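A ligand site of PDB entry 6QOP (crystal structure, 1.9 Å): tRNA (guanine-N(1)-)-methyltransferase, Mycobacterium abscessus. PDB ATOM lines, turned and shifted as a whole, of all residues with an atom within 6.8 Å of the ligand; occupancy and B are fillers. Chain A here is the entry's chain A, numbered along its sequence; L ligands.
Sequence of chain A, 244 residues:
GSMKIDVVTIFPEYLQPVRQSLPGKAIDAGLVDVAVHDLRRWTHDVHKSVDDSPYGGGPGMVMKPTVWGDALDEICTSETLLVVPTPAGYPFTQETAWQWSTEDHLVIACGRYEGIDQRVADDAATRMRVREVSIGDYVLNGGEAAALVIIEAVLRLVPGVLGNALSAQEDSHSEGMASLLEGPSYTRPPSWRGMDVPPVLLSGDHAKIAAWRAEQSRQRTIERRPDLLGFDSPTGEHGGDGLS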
ATOM      1  N   VAL A  84     -22.269  35.509 -26.362  1.00  0.00           N
ATOM      2  CA  VAL A  84     -23.652  35.044 -26.310  1.00  0.00           C
ATOM      3  C   VAL A  84     -23.672  33.536 -26.175  1.00  0.00           C
ATOM      4  O   VAL A  84     -23.511  32.812 -27.153  1.00  0.00           O
ATOM      5  CB  VAL A  84     -24.446  35.443 -27.577  1.00  0.00           C
ATOM      6  CG1 VAL A  84     -25.909  34.993 -27.438  1.00  0.00           C
ATOM      7  CG2 VAL A  84     -24.354  36.940 -27.829  1.00  0.00           C
ATOM      8  N   PRO A  85     -23.820  33.045 -24.936  1.00  0.00           N
ATOM      9  CA  PRO A  85     -23.893  31.591 -24.770  1.00  0.00           C
ATOM     10  C   PRO A  85     -25.178  31.048 -25.403  1.00  0.00           C
ATOM     11  O   PRO A  85     -26.268  31.586 -25.241  1.00  0.00           O
ATOM     12  CB  PRO A  85     -23.896  31.406 -23.249  1.00  0.00           C
ATOM     13  CG  PRO A  85     -23.293  32.691 -22.709  1.00  0.00           C
ATOM     14  CD  PRO A  85     -23.723  33.755 -23.648  1.00  0.00           C
ATOM     15  N   THR A  86     -25.026  29.978 -26.184  1.00  0.00           N
ATOM     16  CA  THR A  86     -26.163  29.389 -26.855  1.00  0.00           C
ATOM     17  C   THR A  86     -25.809  27.984 -27.278  1.00  0.00           C
ATOM     18  O   THR A  86     -24.692  27.755 -27.699  1.00  0.00           O
ATOM     19  CB  THR A  86     -26.609  30.198 -28.097  1.00  0.00           C
ATOM     20  OG1 THR A  86     -27.440  29.353 -28.914  1.00  0.00           O
ATOM     21  CG2 THR A  86     -25.418  30.653 -28.910  1.00  0.00           C
ATOM     22  N   PRO A  87     -26.782  27.068 -27.182  1.00  0.00           N
ATOM     23  CA  PRO A  87     -26.646  25.681 -27.634  1.00  0.00           C
ATOM     24  C   PRO A  87     -26.272  25.594 -29.112  1.00  0.00           C
ATOM     25  O   PRO A  87     -25.711  24.593 -29.523  1.00  0.00           O
ATOM     26  CB  PRO A  87     -28.056  25.095 -27.420  1.00  0.00           C
ATOM     27  CG  PRO A  87     -28.718  26.038 -26.504  1.00  0.00           C
ATOM     28  CD  PRO A  87     -28.127  27.366 -26.677  1.00  0.00           C
ATOM     29  N   ALA A  88     -26.597  26.635 -29.885  1.00  0.00           N
ATOM     30  CA  ALA A  88     -26.289  26.658 -31.312  1.00  0.00           C
ATOM     31  C   ALA A  88     -24.964  27.340 -31.607  1.00  0.00           C
ATOM     32  O   ALA A  88     -24.688  27.672 -32.762  1.00  0.00           O
ATOM     33  CB  ALA A  88     -27.404  27.361 -32.088  1.00  0.00           C
ATOM     34  N   GLY A 111     -29.240  34.306 -22.218  1.00  0.00           N
ATOM     35  CA  GLY A 111     -30.618  34.110 -22.643  1.00  0.00           C
ATOM     36  C   GLY A 111     -31.110  32.694 -22.414  1.00  0.00           C
ATOM     37  O   GLY A 111     -30.321  31.792 -22.148  1.00  0.00           O
ATOM     38  N   ARG A 112     -32.410  32.496 -22.537  1.00  0.00           N
ATOM     39  CA  ARG A 112     -32.990  31.160 -22.420  1.00  0.00           C
ATOM     40  C   ARG A 112     -32.577  30.293 -23.612  1.00  0.00           C
ATOM     41  O   ARG A 112     -32.148  30.815 -24.646  1.00  0.00           O
ATOM     42  CB  ARG A 112     -34.501  31.252 -22.317  1.00  0.00           C
ATOM     43  CG  ARG A 112     -35.142  32.058 -23.440  1.00  0.00           C
ATOM     44  CD  ARG A 112     -36.636  32.284 -23.182  1.00  0.00           C
ATOM     45  NE  ARG A 112     -37.397  31.028 -23.203  1.00  0.00           N
ATOM     46  CZ  ARG A 112     -38.276  30.671 -22.272  1.00  0.00           C
ATOM     47  NH1 ARG A 112     -38.923  29.518 -22.390  1.00  0.00           N
ATOM     48  NH2 ARG A 112     -38.518  31.457 -21.233  1.00  0.00           N
ATOM     49  N   TYR A 113     -32.729  28.975 -23.450  1.00  0.00           N
ATOM     50  CA  TYR A 113     -32.317  27.990 -24.465  1.00  0.00           C
ATOM     51  C   TYR A 113     -32.808  28.351 -25.865  1.00  0.00           C
ATOM     52  O   TYR A 113     -32.042  28.270 -26.829  1.00  0.00           O
ATOM     53  CB  TYR A 113     -32.848  26.592 -24.107  1.00  0.00           C
ATOM     54  CG  TYR A 113     -32.483  25.558 -25.155  1.00  0.00           C
ATOM     55  CD1 TYR A 113     -33.276  25.372 -26.282  1.00  0.00           C
ATOM     56  CD2 TYR A 113     -31.359  24.762 -25.008  1.00  0.00           C
ATOM     57  CE1 TYR A 113     -32.939  24.444 -27.259  1.00  0.00           C
ATOM     58  CE2 TYR A 113     -31.023  23.811 -25.976  1.00  0.00           C
ATOM     59  CZ  TYR A 113     -31.805  23.668 -27.092  1.00  0.00           C
ATOM     60  OH  TYR A 113     -31.471  22.734 -28.047  1.00  0.00           O
ATOM     61  N   GLU A 114     -34.076  28.738 -25.960  1.00  0.00           N
ATOM     62  CA  GLU A 114     -34.718  29.001 -27.232  1.00  0.00           C
ATOM     63  C   GLU A 114     -34.065  30.172 -27.952  1.00  0.00           C
ATOM     64  O   GLU A 114     -34.100  30.240 -29.180  1.00  0.00           O
ATOM     65  CB  GLU A 114     -36.217  29.282 -27.050  1.00  0.00           C
ATOM     66  CG  GLU A 114     -37.059  28.137 -26.482  1.00  0.00           C
ATOM     67  CD  GLU A 114     -36.936  27.990 -24.974  1.00  0.00           C
ATOM     68  OE1 GLU A 114     -36.122  28.706 -24.343  1.00  0.00           O
ATOM     69  OE2 GLU A 114     -37.693  27.167 -24.419  1.00  0.00           O
ATOM     70  N   VAL A 133     -21.381  31.026 -28.456  1.00  0.00           N
ATOM     71  CA  VAL A 133     -20.653  29.802 -28.080  1.00  0.00           C
ATOM     72  C   VAL A 133     -21.480  28.863 -27.233  1.00  0.00           C
ATOM     73  O   VAL A 133     -22.331  29.291 -26.451  1.00  0.00           O
ATOM     74  CB  VAL A 133     -19.328  30.130 -27.312  1.00  0.00           C
ATOM     75  CG1 VAL A 133     -18.321  30.827 -28.235  1.00  0.00           C
ATOM     76  CG2 VAL A 133     -19.604  30.976 -26.079  1.00  0.00           C
ATOM     77  N   SER A 134     -21.244  27.557 -27.403  1.00  0.00           N
ATOM     78  CA  SER A 134     -21.831  26.543 -26.519  1.00  0.00           C
ATOM     79  C   SER A 134     -20.739  25.929 -25.633  1.00  0.00           C
ATOM     80  O   SER A 134     -19.606  25.739 -26.065  1.00  0.00           O
ATOM     81  CB  SER A 134     -22.520  25.456 -27.350  1.00  0.00           C
ATOM     82  OG  SER A 134     -22.635  24.235 -26.624  1.00  0.00           O
ATOM     83  N   ILE A 135     -21.083  25.605 -24.394  1.00  0.00           N
ATOM     84  CA  ILE A 135     -20.104  24.961 -23.519  1.00  0.00           C
ATOM     85  C   ILE A 135     -20.217  23.438 -23.557  1.00  0.00           C
ATOM     86  O   ILE A 135     -19.417  22.724 -22.920  1.00  0.00           O
ATOM     87  CB  ILE A 135     -20.234  25.415 -22.054  1.00  0.00           C
ATOM     88  CG1 ILE A 135     -21.657  25.203 -21.537  1.00  0.00           C
ATOM     89  CG2 ILE A 135     -19.805  26.883 -21.915  1.00  0.00           C
ATOM     90  CD1 ILE A 135     -21.734  25.144 -20.014  1.00  0.00           C
ATOM     91  N   GLY A 136     -21.184  22.923 -24.312  1.00  0.00           N
ATOM     92  CA  GLY A 136     -21.363  21.486 -24.405  1.00  0.00           C
ATOM     93  C   GLY A 136     -22.646  21.053 -25.060  1.00  0.00           C
ATOM     94  O   GLY A 136     -23.572  21.854 -25.274  1.00  0.00           O
ATOM     95  N   ASP A 137     -22.711  19.753 -25.382  1.00  0.00           N
ATOM     96  CA  ASP A 137     -23.857  19.184 -26.059  1.00  0.00           C
ATOM     97  C   ASP A 137     -24.745  18.476 -25.066  1.00  0.00           C
ATOM     98  O   ASP A 137     -24.970  17.264 -25.135  1.00  0.00           O
ATOM     99  CB  ASP A 137     -23.409  18.238 -27.174  1.00  0.00           C
ATOM    100  CG  ASP A 137     -23.027  18.989 -28.433  1.00  0.00           C
ATOM    101  OD1 ASP A 137     -23.485  20.146 -28.601  1.00  0.00           O
ATOM    102  OD2 ASP A 137     -22.250  18.439 -29.238  1.00  0.00           O
ATOM    103  N   TYR A 138     -25.209  19.254 -24.100  1.00  0.00           N
ATOM    104  CA  TYR A 138     -26.260  18.875 -23.194  1.00  0.00           C
ATOM    105  C   TYR A 138     -27.135  20.123 -23.180  1.00  0.00           C
ATOM    106  O   TYR A 138     -26.686  21.196 -23.557  1.00  0.00           O
ATOM    107  CB  TYR A 138     -25.721  18.520 -21.807  1.00  0.00           C
ATOM    108  CG  TYR A 138     -24.493  19.309 -21.456  1.00  0.00           C
ATOM    109  CD1 TYR A 138     -24.588  20.642 -21.042  1.00  0.00           C
ATOM    110  CD2 TYR A 138     -23.242  18.754 -21.562  1.00  0.00           C
ATOM    111  CE1 TYR A 138     -23.454  21.382 -20.742  1.00  0.00           C
ATOM    112  CE2 TYR A 138     -22.103  19.484 -21.254  1.00  0.00           C
ATOM    113  CZ  TYR A 138     -22.211  20.783 -20.850  1.00  0.00           C
ATOM    114  OH  TYR A 138     -21.060  21.498 -20.558  1.00  0.00           O
ATOM    115  N   VAL A 139     -28.381  19.975 -22.738  1.00  0.00           N
ATOM    116  CA  VAL A 139     -29.318  21.077 -22.773  1.00  0.00           C
ATOM    117  C   VAL A 139     -29.505  21.723 -21.408  1.00  0.00           C
ATOM    118  O   VAL A 139     -29.845  21.039 -20.447  1.00  0.00           O
ATOM    119  CB  VAL A 139     -30.693  20.604 -23.289  1.00  0.00           C
ATOM    120  CG1 VAL A 139     -31.663  21.754 -23.351  1.00  0.00           C
ATOM    121  CG2 VAL A 139     -30.541  19.960 -24.665  1.00  0.00           C
ATOM    122  N   LEU A 140     -29.287  23.027 -21.329  1.00  0.00           N
ATOM    123  CA  LEU A 140     -29.598  23.817 -20.133  1.00  0.00           C
ATOM    124  C   LEU A 140     -30.838  24.667 -20.408  1.00  0.00           C
ATOM    125  O   LEU A 140     -31.109  24.981 -21.563  1.00  0.00           O
ATOM    126  CB  LEU A 140     -28.423  24.715 -19.766  1.00  0.00           C
ATOM    127  CG  LEU A 140     -27.067  24.027 -19.675  1.00  0.00           C
ATOM    128  CD1 LEU A 140     -25.970  25.058 -19.523  1.00  0.00           C
ATOM    129  CD2 LEU A 140     -27.042  23.050 -18.515  1.00  0.00           C
ATOM    130  N   ASN A 141     -31.543  25.088 -19.365  1.00  0.00           N
ATOM    131  CA  ASN A 141     -32.710  25.960 -19.534  1.00  0.00           C
ATOM    132  C   ASN A 141     -32.337  27.355 -20.003  1.00  0.00           C
ATOM    133  O   ASN A 141     -33.114  28.030 -20.682  1.00  0.00           O
ATOM    134  CB  ASN A 141     -33.500  26.048 -18.238  1.00  0.00           C
ATOM    135  CG  ASN A 141     -34.570  24.990 -18.150  1.00  0.00           C
ATOM    136  OD1 ASN A 141     -34.973  24.407 -19.159  1.00  0.00           O
ATOM    137  ND2 ASN A 141     -35.035  24.719 -16.933  1.00  0.00           N
ATOM    138  N   GLY A 142     -31.139  27.786 -19.638  1.00  0.00           N
ATOM    139  CA  GLY A 142     -30.716  29.120 -19.992  1.00  0.00           C
ATOM    140  C   GLY A 142     -29.219  29.261 -19.890  1.00  0.00           C
ATOM    141  O   GLY A 142     -28.543  28.331 -19.469  1.00  0.00           O
ATOM    142  N   GLY A 143     -28.703  30.435 -20.256  1.00  0.00           N
ATOM    143  CA  GLY A 143     -27.265  30.626 -20.403  1.00  0.00           C
ATOM    144  C   GLY A 143     -26.487  30.907 -19.125  1.00  0.00           C
ATOM    145  O   GLY A 143     -25.267  30.986 -19.169  1.00  0.00           O
ATOM    146  N   GLU A 144     -27.182  31.040 -17.989  1.00  0.00           N
ATOM    147  CA  GLU A 144     -26.528  31.449 -16.736  1.00  0.00           C
ATOM    148  C   GLU A 144     -25.388  30.517 -16.283  1.00  0.00           C
ATOM    149  O   GLU A 144     -24.307  30.968 -15.924  1.00  0.00           O
ATOM    150  CB  GLU A 144     -27.574  31.549 -15.616  1.00  0.00           C
ATOM    151  CG  GLU A 144     -28.395  32.840 -15.634  1.00  0.00           C
ATOM    152  CD  GLU A 144     -29.426  32.882 -16.763  1.00  0.00           C
ATOM    153  OE1 GLU A 144     -29.845  31.807 -17.242  1.00  0.00           O
ATOM    154  OE2 GLU A 144     -29.820  34.003 -17.152  1.00  0.00           O
ATOM    155  N   ALA A 146     -23.753  28.514 -18.143  1.00  0.00           N
ATOM    156  CA  ALA A 146     -22.711  28.596 -19.170  1.00  0.00           C
ATOM    157  C   ALA A 146     -21.820  29.819 -18.939  1.00  0.00           C
ATOM    158  O   ALA A 146     -20.607  29.775 -19.129  1.00  0.00           O
ATOM    159  CB  ALA A 146     -23.329  28.634 -20.556  1.00  0.00           C
ATOM    160  N   ALA A 147     -22.443  30.917 -18.521  1.00  0.00           N
ATOM    161  CA  ALA A 147     -21.725  32.148 -18.197  1.00  0.00           C
ATOM    162  C   ALA A 147     -20.747  31.927 -17.039  1.00  0.00           C
ATOM    163  O   ALA A 147     -19.626  32.418 -17.064  1.00  0.00           O
ATOM    164  CB  ALA A 147     -22.712  33.272 -17.849  1.00  0.00           C
ATOM    165  N   ILE A 150     -17.825  29.932 -18.394  1.00  0.00           N
ATOM    166  CA  ILE A 150     -16.955  30.819 -19.185  1.00  0.00           C
ATOM    167  C   ILE A 150     -16.161  31.775 -18.283  1.00  0.00           C
ATOM    168  O   ILE A 150     -14.958  31.936 -18.459  1.00  0.00           O
ATOM    169  CB  ILE A 150     -17.778  31.597 -20.206  1.00  0.00           C
ATOM    170  CG1 ILE A 150     -18.379  30.645 -21.237  1.00  0.00           C
ATOM    171  CG2 ILE A 150     -16.915  32.684 -20.891  1.00  0.00           C
ATOM    172  CD1 ILE A 150     -19.502  31.261 -22.072  1.00  0.00           C
HETATM  173  C1  LIG L   1     -26.933  24.771 -23.636  1.00  0.00           C
HETATM  174  F1  LIG L   1     -29.074  26.628 -23.086  1.00  0.00           F
HETATM  175  C2  LIG L   1     -27.828  27.072 -23.236  1.00  0.00           C
HETATM  176  C3  LIG L   1     -27.602  28.436 -23.133  1.00  0.00           C
HETATM  177  C4  LIG L   1     -26.303  28.916 -23.284  1.00  0.00           C
HETATM  178  C5  LIG L   1     -25.244  28.061 -23.552  1.00  0.00           C
HETATM  179  C6  LIG L   1     -25.481  26.654 -23.668  1.00  0.00           C
HETATM  180  N1  LIG L   1     -24.436  25.783 -23.924  1.00  0.00           N
HETATM  181  C7  LIG L   1     -24.646  24.458 -24.039  1.00  0.00           C
HETATM  182  N2  LIG L   1     -25.891  23.950 -23.886  1.00  0.00           N
HETATM  183  O1  LIG L   1     -28.218  24.244 -23.493  1.00  0.00           O
HETATM  184  C8  LIG L   1     -26.738  26.176 -23.518  1.00  0.00           C
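N of Leu 140 is in hydrogen-bond range of O1 of the ligand (2.7 Å).
The backbone carbonyl oxygen (O) of Tyr 138 sits at hydrogen-bond distance from a nitrogen (N2) of the ligand (2.9 Å).
O of Gly 136 lies close to N2 of the ligand (3.4 Å).
A nitrogen (N1) of the ligand lies close to the backbone NH (N) of Ile 135 (3.4 Å).
The side-chain hydroxyl (OH) of Tyr 138 lies within hydrogen-bond range of the backbone carbonyl oxygen (O) of Ile 135 (3.1 Å).
O of Gly 136 sits at hydrogen-bond distance from OG of Ser 134.
N of Ser 134 lies close to O of Thr 86 (3.5 Å).
O of Val 133 lies within hydrogen-bond range of N of Thr 86, at 2.8 Å.
OG1 of Thr 86 lies within hydrogen-bond range of N of Ala 88 (3.0 Å).
The backbone NH of Gly 143 is in hydrogen-bond range of the backbone carbonyl oxygen of Gly 111.
O of Asn 141 is in hydrogen-bond range of N of Tyr 113 (3.0 Å).
C of Pro 85 touches C4 of the ligand, 3.2 Å away.
Thr 86 touches the ligand.
Pro 87 touches the ligand.
Tyr 113 touches the ligand.
Ser 134 touches the ligand (OG to C7, 3.3 Å).
CA of Val 139 touches O1 of the ligand (3.4 Å).
Gly 142 touches the ligand.
Gly 143 touches the ligand.
Ala 146 touches the ligand.
13 residues have an atom within 4 Å of the ligand: Pro 85, Thr 86, Pro 87, Tyr 113, Ser 134, Ile 135, Gly 136, Tyr 138, Val 139, Leu 140, Gly 142, Gly 143 and Ala 146.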
